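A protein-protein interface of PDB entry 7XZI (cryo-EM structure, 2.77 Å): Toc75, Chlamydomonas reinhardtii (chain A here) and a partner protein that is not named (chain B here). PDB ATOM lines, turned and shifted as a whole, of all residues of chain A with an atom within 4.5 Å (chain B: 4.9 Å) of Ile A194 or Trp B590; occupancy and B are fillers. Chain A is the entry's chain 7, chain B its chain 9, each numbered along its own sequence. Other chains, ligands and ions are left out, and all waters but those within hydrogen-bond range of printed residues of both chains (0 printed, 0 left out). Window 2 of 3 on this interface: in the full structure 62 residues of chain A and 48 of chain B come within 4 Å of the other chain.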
ATOM      1  N   THR A 160      -9.878 -17.032 -18.713  1.00  0.00           N
ATOM      2  CA  THR A 160      -8.985 -15.913 -18.453  1.00  0.00           C
ATOM      3  C   THR A 160      -9.762 -14.777 -17.804  1.00  0.00           C
ATOM      4  O   THR A 160     -10.887 -14.467 -18.207  1.00  0.00           O
ATOM      5  CB  THR A 160      -8.314 -15.404 -19.738  1.00  0.00           C
ATOM      6  OG1 THR A 160      -9.311 -15.159 -20.737  1.00  0.00           O
ATOM      7  CG2 THR A 160      -7.309 -16.420 -20.261  1.00  0.00           C
ATOM      8  N   ASN A 161      -9.138 -14.156 -16.801  1.00  0.00           N
ATOM      9  CA  ASN A 161      -9.716 -13.015 -16.088  1.00  0.00           C
ATOM     10  C   ASN A 161     -11.103 -13.349 -15.544  1.00  0.00           C
ATOM     11  O   ASN A 161     -12.045 -12.561 -15.649  1.00  0.00           O
ATOM     12  CB  ASN A 161      -9.758 -11.778 -16.987  1.00  0.00           C
ATOM     13  CG  ASN A 161      -9.901 -10.490 -16.201  1.00  0.00           C
ATOM     14  OD1 ASN A 161      -9.606 -10.442 -15.007  1.00  0.00           O
ATOM     15  ND2 ASN A 161     -10.353  -9.437 -16.870  1.00  0.00           N
ATOM     16  N   ARG A 162     -11.228 -14.535 -14.955  1.00  0.00           N
ATOM     17  CA  ARG A 162     -12.498 -15.042 -14.454  1.00  0.00           C
ATOM     18  C   ARG A 162     -12.502 -15.018 -12.931  1.00  0.00           C
ATOM     19  O   ARG A 162     -11.557 -15.497 -12.296  1.00  0.00           O
ATOM     20  CB  ARG A 162     -12.753 -16.464 -14.957  1.00  0.00           C
ATOM     21  CG  ARG A 162     -14.114 -17.020 -14.575  1.00  0.00           C
ATOM     22  CD  ARG A 162     -14.278 -18.449 -15.058  1.00  0.00           C
ATOM     23  NE  ARG A 162     -13.925 -18.587 -16.464  1.00  0.00           N
ATOM     24  CZ  ARG A 162     -14.747 -18.329 -17.474  1.00  0.00           C
ATOM     25  NH1 ARG A 162     -15.984 -17.906 -17.269  1.00  0.00           N
ATOM     26  NH2 ARG A 162     -14.317 -18.498 -18.720  1.00  0.00           N
ATOM     27  N   HIS A 193     -17.526 -15.997 -13.921  1.00  0.00           N
ATOM     28  CA  HIS A 193     -17.809 -15.187 -15.096  1.00  0.00           C
ATOM     29  C   HIS A 193     -16.746 -14.110 -15.259  1.00  0.00           C
ATOM     30  O   HIS A 193     -16.149 -13.648 -14.282  1.00  0.00           O
ATOM     31  CB  HIS A 193     -19.198 -14.542 -15.017  1.00  0.00           C
ATOM     32  CG  HIS A 193     -20.326 -15.515 -15.180  1.00  0.00           C
ATOM     33  ND1 HIS A 193     -21.031 -16.023 -14.110  1.00  0.00           N
ATOM     34  CD2 HIS A 193     -20.866 -16.075 -16.288  1.00  0.00           C
ATOM     35  CE1 HIS A 193     -21.960 -16.852 -14.553  1.00  0.00           C
ATOM     36  NE2 HIS A 193     -21.880 -16.901 -15.870  1.00  0.00           N
ATOM     37  N   ILE A 194     -16.515 -13.720 -16.514  1.00  0.00           N
ATOM     38  CA  ILE A 194     -15.498 -12.722 -16.816  1.00  0.00           C
ATOM     39  C   ILE A 194     -15.915 -11.361 -16.256  1.00  0.00           C
ATOM     40  O   ILE A 194     -17.106 -11.047 -16.136  1.00  0.00           O
ATOM     41  CB  ILE A 194     -15.255 -12.656 -18.334  1.00  0.00           C
ATOM     42  CG1 ILE A 194     -14.028 -11.803 -18.663  1.00  0.00           C
ATOM     43  CG2 ILE A 194     -16.488 -12.132 -19.057  1.00  0.00           C
ATOM     44  CD1 ILE A 194     -13.728 -11.710 -20.145  1.00  0.00           C
ATOM     45  N   PHE A 195     -14.921 -10.548 -15.900  1.00  0.00           N
ATOM     46  CA  PHE A 195     -15.154  -9.223 -15.345  1.00  0.00           C
ATOM     47  C   PHE A 195     -14.033  -8.290 -15.780  1.00  0.00           C
ATOM     48  O   PHE A 195     -12.970  -8.728 -16.222  1.00  0.00           O
ATOM     49  CB  PHE A 195     -15.246  -9.256 -13.813  1.00  0.00           C
ATOM     50  CG  PHE A 195     -13.941  -9.557 -13.133  1.00  0.00           C
ATOM     51  CD1 PHE A 195     -13.500 -10.863 -13.001  1.00  0.00           C
ATOM     52  CD2 PHE A 195     -13.158  -8.536 -12.621  1.00  0.00           C
ATOM     53  CE1 PHE A 195     -12.301 -11.144 -12.376  1.00  0.00           C
ATOM     54  CE2 PHE A 195     -11.957  -8.811 -11.995  1.00  0.00           C
ATOM     55  CZ  PHE A 195     -11.530 -10.117 -11.872  1.00  0.00           C
ATOM     56  N   GLU A 196     -14.288  -6.988 -15.648  1.00  0.00           N
ATOM     57  CA  GLU A 196     -13.307  -5.964 -15.976  1.00  0.00           C
ATOM     58  C   GLU A 196     -13.343  -4.885 -14.900  1.00  0.00           C
ATOM     59  O   GLU A 196     -14.098  -4.971 -13.926  1.00  0.00           O
ATOM     60  CB  GLU A 196     -13.560  -5.377 -17.369  1.00  0.00           C
ATOM     61  CG  GLU A 196     -14.959  -4.822 -17.572  1.00  0.00           C
ATOM     62  CD  GLU A 196     -15.147  -4.212 -18.947  1.00  0.00           C
ATOM     63  OE1 GLU A 196     -14.132  -3.906 -19.606  1.00  0.00           O
ATOM     64  OE2 GLU A 196     -16.310  -4.044 -19.371  1.00  0.00           O
ATOM     65  N   ASP A 199     -16.758  -3.046 -14.342  1.00  0.00           N
ATOM     66  CA  ASP A 199     -17.702  -3.711 -13.452  1.00  0.00           C
ATOM     67  C   ASP A 199     -17.412  -3.369 -11.997  1.00  0.00           C
ATOM     68  O   ASP A 199     -18.331  -3.104 -11.215  1.00  0.00           O
ATOM     69  CB  ASP A 199     -17.655  -5.223 -13.672  1.00  0.00           C
ATOM     70  CG  ASP A 199     -17.948  -5.614 -15.108  1.00  0.00           C
ATOM     71  OD1 ASP A 199     -18.668  -4.861 -15.797  1.00  0.00           O
ATOM     72  OD2 ASP A 199     -17.457  -6.675 -15.550  1.00  0.00           O
ATOM     73  N   MET B 580     -27.920 -13.031 -27.851  1.00  0.00           N
ATOM     74  CA  MET B 580     -26.958 -13.285 -26.784  1.00  0.00           C
ATOM     75  C   MET B 580     -26.999 -14.740 -26.342  1.00  0.00           C
ATOM     76  O   MET B 580     -25.962 -15.315 -26.002  1.00  0.00           O
ATOM     77  CB  MET B 580     -27.212 -12.354 -25.598  1.00  0.00           C
ATOM     78  CG  MET B 580     -26.981 -10.882 -25.899  1.00  0.00           C
ATOM     79  SD  MET B 580     -25.360 -10.522 -26.599  1.00  0.00           S
ATOM     80  CE  MET B 580     -24.363 -10.432 -25.117  1.00  0.00           C
ATOM     81  N   ASP B 588     -19.015 -17.234 -26.318  1.00  0.00           N
ATOM     82  CA  ASP B 588     -18.555 -15.916 -25.884  1.00  0.00           C
ATOM     83  C   ASP B 588     -18.847 -15.724 -24.400  1.00  0.00           C
ATOM     84  O   ASP B 588     -20.011 -15.824 -23.989  1.00  0.00           O
ATOM     85  CB  ASP B 588     -19.226 -14.823 -26.709  1.00  0.00           C
ATOM     86  CG  ASP B 588     -18.419 -13.538 -26.745  1.00  0.00           C
ATOM     87  OD1 ASP B 588     -17.859 -13.149 -25.698  1.00  0.00           O
ATOM     88  OD2 ASP B 588     -18.339 -12.918 -27.825  1.00  0.00           O
ATOM     89  N   PRO B 589     -17.835 -15.464 -23.566  1.00  0.00           N
ATOM     90  CA  PRO B 589     -18.084 -15.344 -22.118  1.00  0.00           C
ATOM     91  C   PRO B 589     -19.028 -14.214 -21.736  1.00  0.00           C
ATOM     92  O   PRO B 589     -19.814 -14.377 -20.792  1.00  0.00           O
ATOM     93  CB  PRO B 589     -16.680 -15.118 -21.541  1.00  0.00           C
ATOM     94  CG  PRO B 589     -15.751 -15.683 -22.572  1.00  0.00           C
ATOM     95  CD  PRO B 589     -16.401 -15.394 -23.888  1.00  0.00           C
ATOM     96  N   TRP B 590     -18.970 -13.072 -22.426  1.00  0.00           N
ATOM     97  CA  TRP B 590     -19.837 -11.953 -22.065  1.00  0.00           C
ATOM     98  C   TRP B 590     -21.302 -12.298 -22.299  1.00  0.00           C
ATOM     99  O   TRP B 590     -22.170 -11.941 -21.492  1.00  0.00           O
ATOM    100  CB  TRP B 590     -19.442 -10.704 -22.852  1.00  0.00           C
ATOM    101  CG  TRP B 590     -18.037 -10.246 -22.599  1.00  0.00           C
ATOM    102  CD1 TRP B 590     -16.925 -10.580 -23.315  1.00  0.00           C
ATOM    103  CD2 TRP B 590     -17.593  -9.371 -21.555  1.00  0.00           C
ATOM    104  NE1 TRP B 590     -15.818  -9.967 -22.783  1.00  0.00           N
ATOM    105  CE2 TRP B 590     -16.200  -9.218 -21.702  1.00  0.00           C
ATOM    106  CE3 TRP B 590     -18.238  -8.699 -20.511  1.00  0.00           C
ATOM    107  CZ2 TRP B 590     -15.440  -8.424 -20.846  1.00  0.00           C
ATOM    108  CZ3 TRP B 590     -17.482  -7.913 -19.662  1.00  0.00           C
ATOM    109  CH2 TRP B 590     -16.098  -7.781 -19.834  1.00  0.00           C
ATOM    110  N   ALA B 591     -21.594 -12.993 -23.400  1.00  0.00           N
ATOM    111  CA  ALA B 591     -22.958 -13.438 -23.659  1.00  0.00           C
ATOM    112  C   ALA B 591     -23.429 -14.396 -22.573  1.00  0.00           C
ATOM    113  O   ALA B 591     -24.584 -14.335 -22.135  1.00  0.00           O
ATOM    114  CB  ALA B 591     -23.042 -14.093 -25.037  1.00  0.00           C
ATOM    115  N   GLN B 592     -22.542 -15.287 -22.125  1.00  0.00           N
ATOM    116  CA  GLN B 592     -22.864 -16.186 -21.025  1.00  0.00           C
ATOM    117  C   GLN B 592     -23.201 -15.412 -19.758  1.00  0.00           C
ATOM    118  O   GLN B 592     -24.164 -15.736 -19.056  1.00  0.00           O
ATOM    119  CB  GLN B 592     -21.693 -17.140 -20.772  1.00  0.00           C
ATOM    120  CG  GLN B 592     -21.331 -18.016 -21.957  1.00  0.00           C
ATOM    121  CD  GLN B 592     -20.123 -18.890 -21.684  1.00  0.00           C
ATOM    122  OE1 GLN B 592     -19.471 -18.758 -20.648  1.00  0.00           O
ATOM    123  NE2 GLN B 592     -19.818 -19.790 -22.611  1.00  0.00           N
ATOM    124  N   ARG B 593     -22.411 -14.380 -19.448  1.00  0.00           N
ATOM    125  CA  ARG B 593     -22.677 -13.581 -18.254  1.00  0.00           C
ATOM    126  C   ARG B 593     -24.019 -12.865 -18.356  1.00  0.00           C
ATOM    127  O   ARG B 593     -24.799 -12.843 -17.393  1.00  0.00           O
ATOM    128  CB  ARG B 593     -21.546 -12.577 -18.031  1.00  0.00           C
ATOM    129  CG  ARG B 593     -21.624 -11.833 -16.707  1.00  0.00           C
ATOM    130  CD  ARG B 593     -20.298 -11.172 -16.371  1.00  0.00           C
ATOM    131  NE  ARG B 593     -20.078  -9.943 -17.119  1.00  0.00           N
ATOM    132  CZ  ARG B 593     -20.198  -8.723 -16.607  1.00  0.00           C
ATOM    133  NH1 ARG B 593     -20.529  -8.536 -15.340  1.00  0.00           N
ATOM    134  NH2 ARG B 593     -19.977  -7.668 -17.384  1.00  0.00           N
ATOM    135  N   GLU B 594     -24.307 -12.280 -19.522  1.00  0.00           N
ATOM    136  CA  GLU B 594     -25.580 -11.592 -19.711  1.00  0.00           C
ATOM    137  C   GLU B 594     -26.751 -12.555 -19.570  1.00  0.00           C
ATOM    138  O   GLU B 594     -27.750 -12.241 -18.906  1.00  0.00           O
ATOM    139  CB  GLU B 594     -25.612 -10.909 -21.079  1.00  0.00           C
ATOM    140  CG  GLU B 594     -24.520  -9.872 -21.299  1.00  0.00           C
ATOM    141  CD  GLU B 594     -24.720  -8.622 -20.467  1.00  0.00           C
ATOM    142  OE1 GLU B 594     -25.862  -8.372 -20.029  1.00  0.00           O
ATOM    143  OE2 GLU B 594     -23.732  -7.889 -20.251  1.00  0.00           O
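NE of Arg B593 sits close to O of Ile A194. The guanidinium group (NH2) of Arg B593 is in salt-bridge range of the side-chain carboxylate (OD2) of Asp A199, 3.3 Å away.
The side-chain carboxylate of Asp A199 is in hydrogen-bond range of the backbone NH of Glu A196 (3.2 Å). N of Trp B590 lies close to OD1 of Asp B588 (3.5 Å).
Among the printed residues, merely in contact across the chains: His A193 with Arg B593 (3.7 Å), Ile A194 with Pro B589 (3.9 Å), Ile A194 with Trp B590 (3.8 Å) and Glu A196 with Trp B590 (3.8 Å).
Of chain B, only Pro B589 (3.9 Å), Trp B590 (3.8 Å) and Arg B593 (3.2 Å) come within 4 Å of Ile A194. Of chain A, only Ile A194 and Glu A196 come within 4 Å of Trp B590. Printed residues of chain B within 4 Å of Asp A199: Arg B593 (3.3 Å). Of the printed residues of chain B, His A193 touches Arg B593. Of the printed residues of chain A, Arg B593 touches His A193, Ile A194 and Asp A199. Asn A161 touches none of the printed residues of chain B. The nearest printed residue of chain B that does not touch His A193 is Gln B592 (4.1 Å).
Of the 8 printed residues of chain A, 4 touch a printed residue of chain B. Hydrophobic or aromatic side chains of chain A within 4 Å of the printed part of chain B: His A193 and Ile A194. Of the 8 printed residues of chain B, 3 touch a printed residue of chain A. Hydrophobic or aromatic side chains of chain B within 4 Å of the printed part of chain A: Pro B589 and Trp B590. Among the printed residues, Asp or Glu carboxylates within 4 Å of a Lys or Arg side-chain nitrogen of the other chain: Asp A199 with Arg B593 (3.3 Å).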
